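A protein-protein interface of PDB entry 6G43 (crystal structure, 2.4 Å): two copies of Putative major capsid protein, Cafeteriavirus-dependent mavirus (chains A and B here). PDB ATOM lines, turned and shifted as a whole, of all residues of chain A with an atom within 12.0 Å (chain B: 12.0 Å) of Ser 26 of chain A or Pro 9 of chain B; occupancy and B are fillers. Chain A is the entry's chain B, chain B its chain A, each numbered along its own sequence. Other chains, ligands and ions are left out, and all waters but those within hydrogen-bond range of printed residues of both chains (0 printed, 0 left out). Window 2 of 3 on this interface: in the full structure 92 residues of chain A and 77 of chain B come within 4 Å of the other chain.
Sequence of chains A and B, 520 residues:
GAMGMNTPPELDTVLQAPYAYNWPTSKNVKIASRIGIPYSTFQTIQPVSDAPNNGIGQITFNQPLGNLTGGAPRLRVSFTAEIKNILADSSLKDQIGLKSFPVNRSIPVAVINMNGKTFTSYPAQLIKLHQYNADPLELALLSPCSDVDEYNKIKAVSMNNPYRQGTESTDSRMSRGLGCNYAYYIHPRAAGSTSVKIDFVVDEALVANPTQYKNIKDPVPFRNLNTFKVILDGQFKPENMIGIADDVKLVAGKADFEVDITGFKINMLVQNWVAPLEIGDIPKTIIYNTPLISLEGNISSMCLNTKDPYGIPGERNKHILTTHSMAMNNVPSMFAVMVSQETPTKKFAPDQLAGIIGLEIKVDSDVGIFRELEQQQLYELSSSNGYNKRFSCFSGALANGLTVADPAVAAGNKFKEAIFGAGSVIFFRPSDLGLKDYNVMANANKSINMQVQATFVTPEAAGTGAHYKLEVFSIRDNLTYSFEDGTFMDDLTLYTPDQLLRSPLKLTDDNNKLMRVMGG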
ATOM      1  N   ASN A  22       1.154   2.753  12.844  1.00  0.00           N
ATOM      2  CA  ASN A  22       1.202   1.332  13.196  1.00  0.00           C
ATOM      3  C   ASN A  22       0.341   1.132  14.448  1.00  0.00           C
ATOM      4  O   ASN A  22       0.844   1.136  15.571  1.00  0.00           O
ATOM      5  CB  ASN A  22       2.642   0.859  13.436  1.00  0.00           C
ATOM      6  CG  ASN A  22       2.726  -0.627  13.767  1.00  0.00           C
ATOM      7  OD1 ASN A  22       2.007  -1.444  13.191  1.00  0.00           O
ATOM      8  ND2 ASN A  22       3.597  -0.982  14.701  1.00  0.00           N
ATOM      9  N   TRP A  23      -0.963   0.967  14.235  1.00  0.00           N
ATOM     10  CA  TRP A  23      -1.947   0.941  15.326  1.00  0.00           C
ATOM     11  C   TRP A  23      -1.723  -0.282  16.218  1.00  0.00           C
ATOM     12  O   TRP A  23      -1.580  -1.390  15.697  1.00  0.00           O
ATOM     13  CB  TRP A  23      -3.384   0.900  14.783  1.00  0.00           C
ATOM     14  CG  TRP A  23      -3.717   1.968  13.769  1.00  0.00           C
ATOM     15  CD1 TRP A  23      -3.754   1.818  12.414  1.00  0.00           C
ATOM     16  CD2 TRP A  23      -4.066   3.332  14.031  1.00  0.00           C
ATOM     17  NE1 TRP A  23      -4.094   3.003  11.814  1.00  0.00           N
ATOM     18  CE2 TRP A  23      -4.294   3.951  12.782  1.00  0.00           C
ATOM     19  CE3 TRP A  23      -4.204   4.096  15.199  1.00  0.00           C
ATOM     20  CZ2 TRP A  23      -4.654   5.298  12.664  1.00  0.00           C
ATOM     21  CZ3 TRP A  23      -4.565   5.440  15.081  1.00  0.00           C
ATOM     22  CH2 TRP A  23      -4.785   6.024  13.820  1.00  0.00           C
ATOM     23  N   PRO A  24      -1.660  -0.089  17.555  1.00  0.00           N
ATOM     24  CA  PRO A  24      -1.630  -1.262  18.430  1.00  0.00           C
ATOM     25  C   PRO A  24      -2.957  -2.026  18.403  1.00  0.00           C
ATOM     26  O   PRO A  24      -4.016  -1.440  18.635  1.00  0.00           O
ATOM     27  CB  PRO A  24      -1.353  -0.677  19.820  1.00  0.00           C
ATOM     28  CG  PRO A  24      -0.796   0.680  19.584  1.00  0.00           C
ATOM     29  CD  PRO A  24      -1.387   1.157  18.296  1.00  0.00           C
ATOM     30  N   THR A  25      -2.877  -3.317  18.090  1.00  0.00           N
ATOM     31  CA  THR A  25      -4.031  -4.206  18.002  1.00  0.00           C
ATOM     32  C   THR A  25      -3.665  -5.542  18.639  1.00  0.00           C
ATOM     33  O   THR A  25      -2.511  -5.769  19.011  1.00  0.00           O
ATOM     34  CB  THR A  25      -4.446  -4.454  16.535  1.00  0.00           C
ATOM     35  OG1 THR A  25      -3.401  -5.152  15.843  1.00  0.00           O
ATOM     36  CG2 THR A  25      -4.740  -3.141  15.814  1.00  0.00           C
ATOM     37  N   SER A  26      -4.651  -6.430  18.741  1.00  0.00           N
ATOM     38  CA  SER A  26      -4.429  -7.803  19.200  1.00  0.00           C
ATOM     39  C   SER A  26      -3.443  -8.599  18.330  1.00  0.00           C
ATOM     40  O   SER A  26      -2.823  -9.546  18.812  1.00  0.00           O
ATOM     41  CB  SER A  26      -5.764  -8.553  19.283  1.00  0.00           C
ATOM     42  OG  SER A  26      -6.385  -8.637  18.013  1.00  0.00           O
ATOM     43  N   LYS A  27      -3.314  -8.220  17.058  1.00  0.00           N
ATOM     44  CA  LYS A  27      -2.384  -8.864  16.128  1.00  0.00           C
ATOM     45  C   LYS A  27      -0.913  -8.466  16.294  1.00  0.00           C
ATOM     46  O   LYS A  27      -0.037  -9.204  15.842  1.00  0.00           O
ATOM     47  CB  LYS A  27      -2.828  -8.593  14.686  1.00  0.00           C
ATOM     48  CG  LYS A  27      -4.148  -9.254  14.321  1.00  0.00           C
ATOM     49  CD  LYS A  27      -4.601  -8.867  12.923  1.00  0.00           C
ATOM     50  CE  LYS A  27      -5.929  -9.520  12.568  1.00  0.00           C
ATOM     51  NZ  LYS A  27      -6.405  -9.108  11.216  1.00  0.00           N
ATOM     52  N   ASN A  28      -0.638  -7.314  16.914  1.00  0.00           N
ATOM     53  CA  ASN A  28       0.750  -6.836  17.096  1.00  0.00           C
ATOM     54  C   ASN A  28       1.134  -6.382  18.519  1.00  0.00           C
ATOM     55  O   ASN A  28       2.170  -5.738  18.699  1.00  0.00           O
ATOM     56  CB  ASN A  28       1.069  -5.734  16.064  1.00  0.00           C
ATOM     57  CG  ASN A  28       0.288  -4.447  16.294  1.00  0.00           C
ATOM     58  OD1 ASN A  28      -0.555  -4.355  17.187  1.00  0.00           O
ATOM     59  ND2 ASN A  28       0.572  -3.438  15.480  1.00  0.00           N
ATOM     60  N   VAL A  29       0.321  -6.731  19.518  1.00  0.00           N
ATOM     61  CA  VAL A  29       0.601  -6.395  20.919  1.00  0.00           C
ATOM     62  C   VAL A  29       0.682  -7.675  21.744  1.00  0.00           C
ATOM     63  O   VAL A  29      -0.062  -8.628  21.505  1.00  0.00           O
ATOM     64  CB  VAL A  29      -0.465  -5.442  21.515  1.00  0.00           C
ATOM     65  CG1 VAL A  29      -0.253  -5.230  23.012  1.00  0.00           C
ATOM     66  CG2 VAL A  29      -0.427  -4.096  20.805  1.00  0.00           C
ATOM     67  N   LYS A  30       1.601  -7.683  22.707  1.00  0.00           N
ATOM     68  CA  LYS A  30       1.720  -8.754  23.690  1.00  0.00           C
ATOM     69  C   LYS A  30       1.988  -8.140  25.062  1.00  0.00           C
ATOM     70  O   LYS A  30       2.622  -7.087  25.162  1.00  0.00           O
ATOM     71  CB  LYS A  30       2.843  -9.717  23.303  1.00  0.00           C
ATOM     72  CG  LYS A  30       2.531 -10.545  22.066  1.00  0.00           C
ATOM     73  CD  LYS A  30       3.651 -11.512  21.718  1.00  0.00           C
ATOM     74  CE  LYS A  30       3.266 -12.376  20.526  1.00  0.00           C
ATOM     75  NZ  LYS A  30       4.405 -13.197  20.035  1.00  0.00           N
ATOM     76  N   ILE A  31       1.483  -8.791  26.107  1.00  0.00           N
ATOM     77  CA  ILE A  31       1.683  -8.337  27.481  1.00  0.00           C
ATOM     78  C   ILE A  31       2.834  -9.116  28.096  1.00  0.00           C
ATOM     79  O   ILE A  31       2.881 -10.341  28.004  1.00  0.00           O
ATOM     80  CB  ILE A  31       0.418  -8.522  28.345  1.00  0.00           C
ATOM     81  CG1 ILE A  31      -0.819  -7.920  27.660  1.00  0.00           C
ATOM     82  CG2 ILE A  31       0.613  -7.897  29.723  1.00  0.00           C
ATOM     83  CD1 ILE A  31      -0.693  -6.464  27.256  1.00  0.00           C
ATOM     84  N   ALA A  32       3.755  -8.397  28.731  1.00  0.00           N
ATOM     85  CA  ALA A  32       4.921  -9.006  29.353  1.00  0.00           C
ATOM     86  C   ALA A  32       4.728  -9.146  30.857  1.00  0.00           C
ATOM     87  O   ALA A  32       4.072  -8.319  31.489  1.00  0.00           O
ATOM     88  CB  ALA A  32       6.163  -8.181  29.061  1.00  0.00           C
ATOM     89  N   ASN B   6     -19.389  -5.199  23.371  1.00  0.00           N
ATOM     90  CA  ASN B   6     -17.902  -5.064  23.210  1.00  0.00           C
ATOM     91  C   ASN B   6     -17.143  -5.696  24.379  1.00  0.00           C
ATOM     92  O   ASN B   6     -17.556  -5.581  25.534  1.00  0.00           O
ATOM     93  CB  ASN B   6     -17.488  -3.593  23.066  1.00  0.00           C
ATOM     94  CG  ASN B   6     -18.031  -2.952  21.797  1.00  0.00           C
ATOM     95  OD1 ASN B   6     -17.703  -3.376  20.690  1.00  0.00           O
ATOM     96  ND2 ASN B   6     -18.859  -1.922  21.952  1.00  0.00           N
ATOM     97  N   THR B   7     -16.033  -6.357  24.060  1.00  0.00           N
ATOM     98  CA  THR B   7     -15.188  -7.016  25.051  1.00  0.00           C
ATOM     99  C   THR B   7     -13.715  -6.886  24.622  1.00  0.00           C
ATOM    100  O   THR B   7     -13.423  -6.940  23.421  1.00  0.00           O
ATOM    101  CB  THR B   7     -15.592  -8.502  25.237  1.00  0.00           C
ATOM    102  OG1 THR B   7     -14.769  -9.108  26.240  1.00  0.00           O
ATOM    103  CG2 THR B   7     -15.476  -9.300  23.932  1.00  0.00           C
ATOM    104  N   PRO B   8     -12.786  -6.696  25.589  1.00  0.00           N
ATOM    105  CA  PRO B   8     -11.367  -6.622  25.211  1.00  0.00           C
ATOM    106  C   PRO B   8     -10.854  -7.933  24.605  1.00  0.00           C
ATOM    107  O   PRO B   8     -11.183  -9.003  25.120  1.00  0.00           O
ATOM    108  CB  PRO B   8     -10.650  -6.343  26.541  1.00  0.00           C
ATOM    109  CG  PRO B   8     -11.696  -5.804  27.448  1.00  0.00           C
ATOM    110  CD  PRO B   8     -12.974  -6.466  27.034  1.00  0.00           C
ATOM    111  N   PRO B   9     -10.056  -7.852  23.521  1.00  0.00           N
ATOM    112  CA  PRO B   9      -9.549  -9.064  22.881  1.00  0.00           C
ATOM    113  C   PRO B   9      -8.452  -9.740  23.704  1.00  0.00           C
ATOM    114  O   PRO B   9      -7.796  -9.083  24.517  1.00  0.00           O
ATOM    115  CB  PRO B   9      -8.988  -8.545  21.556  1.00  0.00           C
ATOM    116  CG  PRO B   9      -8.542  -7.161  21.870  1.00  0.00           C
ATOM    117  CD  PRO B   9      -9.515  -6.634  22.887  1.00  0.00           C
ATOM    118  N   GLU B  10      -8.275 -11.045  23.495  1.00  0.00           N
ATOM    119  CA  GLU B  10      -7.214 -11.803  24.161  1.00  0.00           C
ATOM    120  C   GLU B  10      -5.853 -11.384  23.621  1.00  0.00           C
ATOM    121  O   GLU B  10      -5.661 -11.303  22.405  1.00  0.00           O
ATOM    122  CB  GLU B  10      -7.390 -13.319  23.979  1.00  0.00           C
ATOM    123  CG  GLU B  10      -8.113 -14.011  25.128  1.00  0.00           C
ATOM    124  CD  GLU B  10      -8.069 -15.529  25.024  1.00  0.00           C
ATOM    125  OE1 GLU B  10      -6.960 -16.090  24.872  1.00  0.00           O
ATOM    126  OE2 GLU B  10      -9.144 -16.163  25.105  1.00  0.00           O
ATOM    127  N   LEU B  11      -4.924 -11.124  24.537  1.00  0.00           N
ATOM    128  CA  LEU B  11      -3.556 -10.754  24.197  1.00  0.00           C
ATOM    129  C   LEU B  11      -2.619 -11.839  24.699  1.00  0.00           C
ATOM    130  O   LEU B  11      -2.751 -12.300  25.836  1.00  0.00           O
ATOM    131  CB  LEU B  11      -3.196  -9.410  24.830  1.00  0.00           C
ATOM    132  CG  LEU B  11      -4.054  -8.212  24.406  1.00  0.00           C
ATOM    133  CD1 LEU B  11      -3.698  -6.979  25.224  1.00  0.00           C
ATOM    134  CD2 LEU B  11      -3.893  -7.928  22.921  1.00  0.00           C
ATOM    135  N   ASP B  12      -1.680 -12.243  23.846  1.00  0.00           N
ATOM    136  CA  ASP B  12      -0.696 -13.269  24.193  1.00  0.00           C
ATOM    137  C   ASP B  12       0.328 -12.704  25.165  1.00  0.00           C
ATOM    138  O   ASP B  12       0.559 -11.491  25.204  1.00  0.00           O
ATOM    139  CB  ASP B  12       0.022 -13.786  22.942  1.00  0.00           C
ATOM    140  CG  ASP B  12      -0.916 -14.463  21.954  1.00  0.00           C
ATOM    141  OD1 ASP B  12      -1.920 -15.075  22.386  1.00  0.00           O
ATOM    142  OD2 ASP B  12      -0.640 -14.381  20.739  1.00  0.00           O
ATOM    143  N   THR B  13       0.936 -13.598  25.942  1.00  0.00           N
ATOM    144  CA  THR B  13       1.886 -13.217  26.980  1.00  0.00           C
ATOM    145  C   THR B  13       3.311 -13.644  26.638  1.00  0.00           C
ATOM    146  O   THR B  13       3.523 -14.594  25.880  1.00  0.00           O
ATOM    147  CB  THR B  13       1.485 -13.807  28.346  1.00  0.00           C
ATOM    148  OG1 THR B  13       1.219 -15.208  28.209  1.00  0.00           O
ATOM    149  CG2 THR B  13       0.243 -13.108  28.883  1.00  0.00           C
ATOM    150  N   VAL B  14       4.277 -12.907  27.185  1.00  0.00           N
ATOM    151  CA  VAL B  14       5.696 -13.258  27.114  1.00  0.00           C
ATOM    152  C   VAL B  14       6.343 -13.049  28.481  1.00  0.00           C
ATOM    153  O   VAL B  14       5.879 -12.234  29.280  1.00  0.00           O
ATOM    154  CB  VAL B  14       6.457 -12.446  26.035  1.00  0.00           C
ATOM    155  CG1 VAL B  14       5.948 -12.803  24.646  1.00  0.00           C
ATOM    156  CG2 VAL B  14       6.352 -10.940  26.276  1.00  0.00           C
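The backbone carbonyl oxygen (O) of Asp 12 of chain B lies within hydrogen-bond range of the backbone NH (N) of Ile 31 of chain A (3.0 Å). The backbone NH of Val 14 of chain B lies within hydrogen-bond range of the backbone carbonyl oxygen of Ile 31 of chain A (3.0 Å).
No residue of chain B comes within 4 Å of Thr 25 of chain A. Ser 26 of chain A touches just these residues of chain B: Pro 9 (3.9 Å) and Leu 11 (3.8 Å). No residue of chain B comes within 4 Å of Asn 28 of chain A. Of the printed residues of chain B, Lys 30 of chain A touches Asp 12 (3.3 Å) and Val 14 (3.9 Å). Of the printed residues of chain B, Ile 31 of chain A touches Leu 11, Asp 12, Thr 13 and Val 14. Printed residues of chain B within 4 Å of Ala 32 of chain A: Val 14. No residue of chain A comes within 4 Å of Thr 7 of chain B. No residue of chain A comes within 4 Å of Pro 8 of chain B. Of chain A, only Ser 26 comes within 4 Å of Pro 9 of chain B. No residue of chain A comes within 4 Å of Glu 10 of chain B. Of the printed residues of chain A, Leu 11 of chain B touches Ser 26 and Ile 31. Printed residues of chain A within 4 Å of Val 14 of chain B: Lys 30 (3.9 Å), Ile 31 (3.0 Å) and Ala 32 (3.4 Å). The nearest residue of chain A that does not touch Pro 9 of chain B is Thr 25 of chain A (6.1 Å).
Of the 11 printed residues of chain A, 4 touch a printed residue of chain B. Hydrophobic or aromatic side chains of chain A that line the printed part of chain B: Ile 31 and Ala 32. Printed residues of chain B that touch a printed residue of chain A: Pro 9, Leu 11, Asp 12, Thr 13 and Val 14. Hydrophobic or aromatic side chains of chain B that line the printed part of chain A: Pro 9, Leu 11 and Val 14. Among the printed residues, 9 pairs touch across the chains. Among the printed residues, no Asp or Glu carboxylate lies within 4 Å of a Lys or Arg side-chain nitrogen of the other chain.
No position is printed for both chains.
Pro 9 of chain B touches Ser 26 of chain A (CB to CB, 3.9 Å). Ser 26 of chain A touches Leu 11 of chain B (CA to CD2, 3.8 Å). O of Asp 12 of chain B touches CA of Lys 30 of chain A, at 3.3 Å. Val 14 of chain B touches Lys 30 of chain A (CG1 to CD, 3.9 Å). Leu 11 of chain B touches Ile 31 of chain A (CD1 to CD1, 3.7 Å). CA of Thr 13 of chain B touches O of Ile 31 of chain A (3.2 Å). CA of Ala 32 of chain A touches O of Val 14 of chain B (3.4 Å).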
